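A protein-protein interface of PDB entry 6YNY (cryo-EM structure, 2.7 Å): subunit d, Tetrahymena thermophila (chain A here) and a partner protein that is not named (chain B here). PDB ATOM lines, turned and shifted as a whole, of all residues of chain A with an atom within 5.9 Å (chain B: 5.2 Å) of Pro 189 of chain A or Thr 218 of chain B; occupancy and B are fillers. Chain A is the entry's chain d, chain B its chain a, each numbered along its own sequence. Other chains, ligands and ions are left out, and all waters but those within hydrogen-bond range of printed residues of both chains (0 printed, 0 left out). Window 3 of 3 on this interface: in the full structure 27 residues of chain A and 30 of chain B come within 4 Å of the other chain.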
ATOM      1  N   ASN A 186      21.112  18.673   9.939  1.00  0.00           N
ATOM      2  CA  ASN A 186      19.801  18.420  10.530  1.00  0.00           C
ATOM      3  C   ASN A 186      18.831  19.521  10.106  1.00  0.00           C
ATOM      4  O   ASN A 186      18.254  20.244  10.917  1.00  0.00           O
ATOM      5  CB  ASN A 186      19.911  18.319  12.045  1.00  0.00           C
ATOM      6  CG  ASN A 186      20.389  16.964  12.505  1.00  0.00           C
ATOM      7  OD1 ASN A 186      19.604  16.027  12.637  1.00  0.00           O
ATOM      8  ND2 ASN A 186      21.682  16.850  12.758  1.00  0.00           N
ATOM      9  N   TYR A 187      18.671  19.638   8.790  1.00  0.00           N
ATOM     10  CA  TYR A 187      17.863  20.686   8.190  1.00  0.00           C
ATOM     11  C   TYR A 187      16.391  20.314   8.093  1.00  0.00           C
ATOM     12  O   TYR A 187      15.657  20.927   7.310  1.00  0.00           O
ATOM     13  CB  TYR A 187      18.411  21.056   6.809  1.00  0.00           C
ATOM     14  CG  TYR A 187      18.545  19.915   5.831  1.00  0.00           C
ATOM     15  CD1 TYR A 187      19.784  19.371   5.544  1.00  0.00           C
ATOM     16  CD2 TYR A 187      17.439  19.398   5.181  1.00  0.00           C
ATOM     17  CE1 TYR A 187      19.917  18.342   4.647  1.00  0.00           C
ATOM     18  CE2 TYR A 187      17.561  18.365   4.282  1.00  0.00           C
ATOM     19  CZ  TYR A 187      18.803  17.840   4.018  1.00  0.00           C
ATOM     20  OH  TYR A 187      18.936  16.810   3.121  1.00  0.00           O
ATOM     21  N   ILE A 188      15.945  19.328   8.863  1.00  0.00           N
ATOM     22  CA  ILE A 188      14.524  19.042   9.028  1.00  0.00           C
ATOM     23  C   ILE A 188      14.044  19.818  10.253  1.00  0.00           C
ATOM     24  O   ILE A 188      14.498  19.521  11.370  1.00  0.00           O
ATOM     25  CB  ILE A 188      14.260  17.542   9.182  1.00  0.00           C
ATOM     26  CG1 ILE A 188      14.779  16.789   7.960  1.00  0.00           C
ATOM     27  CG2 ILE A 188      12.786  17.299   9.360  1.00  0.00           C
ATOM     28  CD1 ILE A 188      14.652  15.296   8.063  1.00  0.00           C
ATOM     29  N   PRO A 189      13.158  20.797  10.099  1.00  0.00           N
ATOM     30  CA  PRO A 189      12.827  21.666  11.234  1.00  0.00           C
ATOM     31  C   PRO A 189      12.141  20.910  12.361  1.00  0.00           C
ATOM     32  O   PRO A 189      11.207  20.135  12.140  1.00  0.00           O
ATOM     33  CB  PRO A 189      11.910  22.721  10.607  1.00  0.00           C
ATOM     34  CG  PRO A 189      11.369  22.094   9.403  1.00  0.00           C
ATOM     35  CD  PRO A 189      12.433  21.194   8.884  1.00  0.00           C
ATOM     36  N   GLY A 190      12.619  21.146  13.580  1.00  0.00           N
ATOM     37  CA  GLY A 190      12.025  20.563  14.763  1.00  0.00           C
ATOM     38  C   GLY A 190      12.406  19.133  15.051  1.00  0.00           C
ATOM     39  O   GLY A 190      11.730  18.474  15.845  1.00  0.00           O
ATOM     40  N   ALA A 191      13.477  18.629  14.441  1.00  0.00           N
ATOM     41  CA  ALA A 191      13.857  17.238  14.653  1.00  0.00           C
ATOM     42  C   ALA A 191      14.467  17.031  16.031  1.00  0.00           C
ATOM     43  O   ALA A 191      14.246  15.991  16.663  1.00  0.00           O
ATOM     44  CB  ALA A 191      14.829  16.793  13.565  1.00  0.00           C
ATOM     45  N   ASP A 193      13.888  19.016  18.645  1.00  0.00           N
ATOM     46  CA  ASP A 193      13.030  19.621  19.652  1.00  0.00           C
ATOM     47  C   ASP A 193      12.041  18.572  20.140  1.00  0.00           C
ATOM     48  O   ASP A 193      11.293  17.998  19.343  1.00  0.00           O
ATOM     49  CB  ASP A 193      12.299  20.838  19.092  1.00  0.00           C
ATOM     50  CG  ASP A 193      13.234  21.984  18.776  1.00  0.00           C
ATOM     51  OD1 ASP A 193      13.874  21.957  17.706  1.00  0.00           O
ATOM     52  OD2 ASP A 193      13.332  22.914  19.601  1.00  0.00           O
ATOM     53  N   ASN A 196       7.869  19.846  19.190  1.00  0.00           N
ATOM     54  CA  ASN A 196       7.903  20.685  17.996  1.00  0.00           C
ATOM     55  C   ASN A 196       6.524  21.318  17.811  1.00  0.00           C
ATOM     56  O   ASN A 196       5.739  20.960  16.931  1.00  0.00           O
ATOM     57  CB  ASN A 196       8.326  19.874  16.782  1.00  0.00           C
ATOM     58  CG  ASN A 196       8.462  20.716  15.542  1.00  0.00           C
ATOM     59  OD1 ASN A 196       8.529  21.940  15.611  1.00  0.00           O
ATOM     60  ND2 ASN A 196       8.504  20.062  14.393  1.00  0.00           N
ATOM     61  N   ILE A 212       7.714  15.193  12.497  1.00  0.00           N
ATOM     62  CA  ILE A 212       8.960  14.480  12.274  1.00  0.00           C
ATOM     63  C   ILE A 212       9.350  13.739  13.541  1.00  0.00           C
ATOM     64  O   ILE A 212       9.131  14.221  14.661  1.00  0.00           O
ATOM     65  CB  ILE A 212      10.064  15.452  11.829  1.00  0.00           C
ATOM     66  CG1 ILE A 212      11.235  14.685  11.222  1.00  0.00           C
ATOM     67  CG2 ILE A 212      10.539  16.288  12.991  1.00  0.00           C
ATOM     68  CD1 ILE A 212      10.952  14.153   9.850  1.00  0.00           C
ATOM     69  N   ALA B 214       8.322  23.989   2.737  1.00  0.00           N
ATOM     70  CA  ALA B 214       9.513  23.168   2.909  1.00  0.00           C
ATOM     71  C   ALA B 214       9.339  22.184   4.056  1.00  0.00           C
ATOM     72  O   ALA B 214       9.809  21.044   3.980  1.00  0.00           O
ATOM     73  CB  ALA B 214      10.729  24.059   3.143  1.00  0.00           C
ATOM     74  N   ALA B 215       8.662  22.606   5.123  1.00  0.00           N
ATOM     75  CA  ALA B 215       8.417  21.716   6.248  1.00  0.00           C
ATOM     76  C   ALA B 215       7.438  20.609   5.890  1.00  0.00           C
ATOM     77  O   ALA B 215       7.534  19.502   6.430  1.00  0.00           O
ATOM     78  CB  ALA B 215       7.895  22.515   7.436  1.00  0.00           C
ATOM     79  N   SER B 216       6.490  20.886   4.996  1.00  0.00           N
ATOM     80  CA  SER B 216       5.535  19.868   4.583  1.00  0.00           C
ATOM     81  C   SER B 216       6.176  18.798   3.715  1.00  0.00           C
ATOM     82  O   SER B 216       5.598  17.720   3.554  1.00  0.00           O
ATOM     83  CB  SER B 216       4.375  20.512   3.832  1.00  0.00           C
ATOM     84  OG  SER B 216       4.810  21.081   2.612  1.00  0.00           O
ATOM     85  N   GLY B 217       7.350  19.070   3.158  1.00  0.00           N
ATOM     86  CA  GLY B 217       8.033  18.109   2.323  1.00  0.00           C
ATOM     87  C   GLY B 217       9.039  17.272   3.081  1.00  0.00           C
ATOM     88  O   GLY B 217       9.095  16.051   2.912  1.00  0.00           O
ATOM     89  N   THR B 218       9.843  17.923   3.920  1.00  0.00           N
ATOM     90  CA  THR B 218      10.834  17.195   4.702  1.00  0.00           C
ATOM     91  C   THR B 218      10.182  16.276   5.724  1.00  0.00           C
ATOM     92  O   THR B 218      10.789  15.281   6.134  1.00  0.00           O
ATOM     93  CB  THR B 218      11.777  18.171   5.405  1.00  0.00           C
ATOM     94  OG1 THR B 218      11.033  19.016   6.291  1.00  0.00           O
ATOM     95  CG2 THR B 218      12.515  19.015   4.391  1.00  0.00           C
ATOM     96  N   VAL B 219       8.958  16.590   6.152  1.00  0.00           N
ATOM     97  CA  VAL B 219       8.260  15.724   7.090  1.00  0.00           C
ATOM     98  C   VAL B 219       7.830  14.424   6.432  1.00  0.00           C
ATOM     99  O   VAL B 219       7.598  13.430   7.126  1.00  0.00           O
ATOM    100  CB  VAL B 219       7.039  16.442   7.687  1.00  0.00           C
ATOM    101  CG1 VAL B 219       5.943  16.573   6.657  1.00  0.00           C
ATOM    102  CG2 VAL B 219       6.535  15.702   8.897  1.00  0.00           C
ATOM    103  N   GLU B 220       7.720  14.403   5.107  1.00  0.00           N
ATOM    104  CA  GLU B 220       7.345  13.185   4.410  1.00  0.00           C
ATOM    105  C   GLU B 220       8.448  12.143   4.421  1.00  0.00           C
ATOM    106  O   GLU B 220       8.235  11.037   3.916  1.00  0.00           O
ATOM    107  CB  GLU B 220       6.945  13.509   2.974  1.00  0.00           C
ATOM    108  CG  GLU B 220       5.895  14.593   2.864  1.00  0.00           C
ATOM    109  CD  GLU B 220       4.618  14.254   3.607  1.00  0.00           C
ATOM    110  OE1 GLU B 220       4.392  13.062   3.897  1.00  0.00           O
ATOM    111  OE2 GLU B 220       3.838  15.181   3.904  1.00  0.00           O
ATOM    112  N   ALA B 221       9.617  12.468   4.972  1.00  0.00           N
ATOM    113  CA  ALA B 221      10.628  11.449   5.205  1.00  0.00           C
ATOM    114  C   ALA B 221      10.101  10.328   6.085  1.00  0.00           C
ATOM    115  O   ALA B 221      10.644   9.220   6.052  1.00  0.00           O
ATOM    116  CB  ALA B 221      11.859  12.079   5.847  1.00  0.00           C
ATOM    117  N   GLU B 222       9.057  10.594   6.872  1.00  0.00           N
ATOM    118  CA  GLU B 222       8.434   9.557   7.678  1.00  0.00           C
ATOM    119  C   GLU B 222       7.679   8.542   6.834  1.00  0.00           C
ATOM    120  O   GLU B 222       7.333   7.471   7.342  1.00  0.00           O
ATOM    121  CB  GLU B 222       7.490  10.187   8.698  1.00  0.00           C
ATOM    122  CG  GLU B 222       8.170  11.145   9.647  1.00  0.00           C
ATOM    123  CD  GLU B 222       9.185  10.462  10.542  1.00  0.00           C
ATOM    124  OE1 GLU B 222       9.075   9.234  10.736  1.00  0.00           O
ATOM    125  OE2 GLU B 222      10.094  11.149  11.049  1.00  0.00           O
ATOM    126  N   ILE B 228      15.976  11.386   2.329  1.00  0.00           N
ATOM    127  CA  ILE B 228      15.520  12.633   1.726  1.00  0.00           C
ATOM    128  C   ILE B 228      16.712  13.469   1.286  1.00  0.00           C
ATOM    129  O   ILE B 228      16.613  14.253   0.336  1.00  0.00           O
ATOM    130  CB  ILE B 228      14.607  13.399   2.704  1.00  0.00           C
ATOM    131  CG1 ILE B 228      14.031  14.661   2.058  1.00  0.00           C
ATOM    132  CG2 ILE B 228      15.353  13.788   3.940  1.00  0.00           C
ATOM    133  CD1 ILE B 228      13.060  14.404   0.948  1.00  0.00           C
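The backbone carbonyl oxygen of Ala 214 of chain B lies within hydrogen-bond range of the side-chain hydroxyl of Thr 218 of chain B, 3.3 Å away.
CG2 of Ile 188 of chain A touches OG1 of Thr 218 of chain B, 3.9 Å away. Thr 218 of chain B touches Pro 189 of chain A (OG1 to CD, 3.7 Å). O of Thr 218 of chain B touches CD1 of Ile 212 of chain A (3.9 Å). N of Ile 212 of chain A touches CG2 of Val 219 of chain B (3.8 Å). CD1 of Ile 212 of chain A touches OE2 of Glu 222 of chain B (3.3 Å).
Of the 10 printed residues of chain B, 3 touch a printed residue of chain A. Hydrophobic or aromatic side chains of chain B within 4 Å of the printed part of chain A: Val 219. Hydrophobic or aromatic side chains of chain A that line the printed part of chain B: Ile 188, Pro 189 and Ile 212. Along chain A the printed residues that touch a printed residue of chain B span positions 188 to 212.
Of the printed residues of chain B, Pro 189 of chain A touches Thr 218. Thr 218 of chain B touches just these residues of chain A: Ile 188 (3.9 Å), Pro 189 (3.7 Å) and Ile 212 (3.9 Å). Printed residues of chain A within 4 Å of Val 219 of chain B: Ile 212 (3.8 Å). Printed residues of chain A within 4 Å of Glu 222 of chain B: Ile 212 (3.3 Å). Printed residues of chain B within 4 Å of Ile 188 of chain A: Thr 218. Printed residues of chain B within 4 Å of Ile 212 of chain A: Thr 218 (3.9 Å), Val 219 (3.8 Å) and Glu 222 (3.3 Å).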
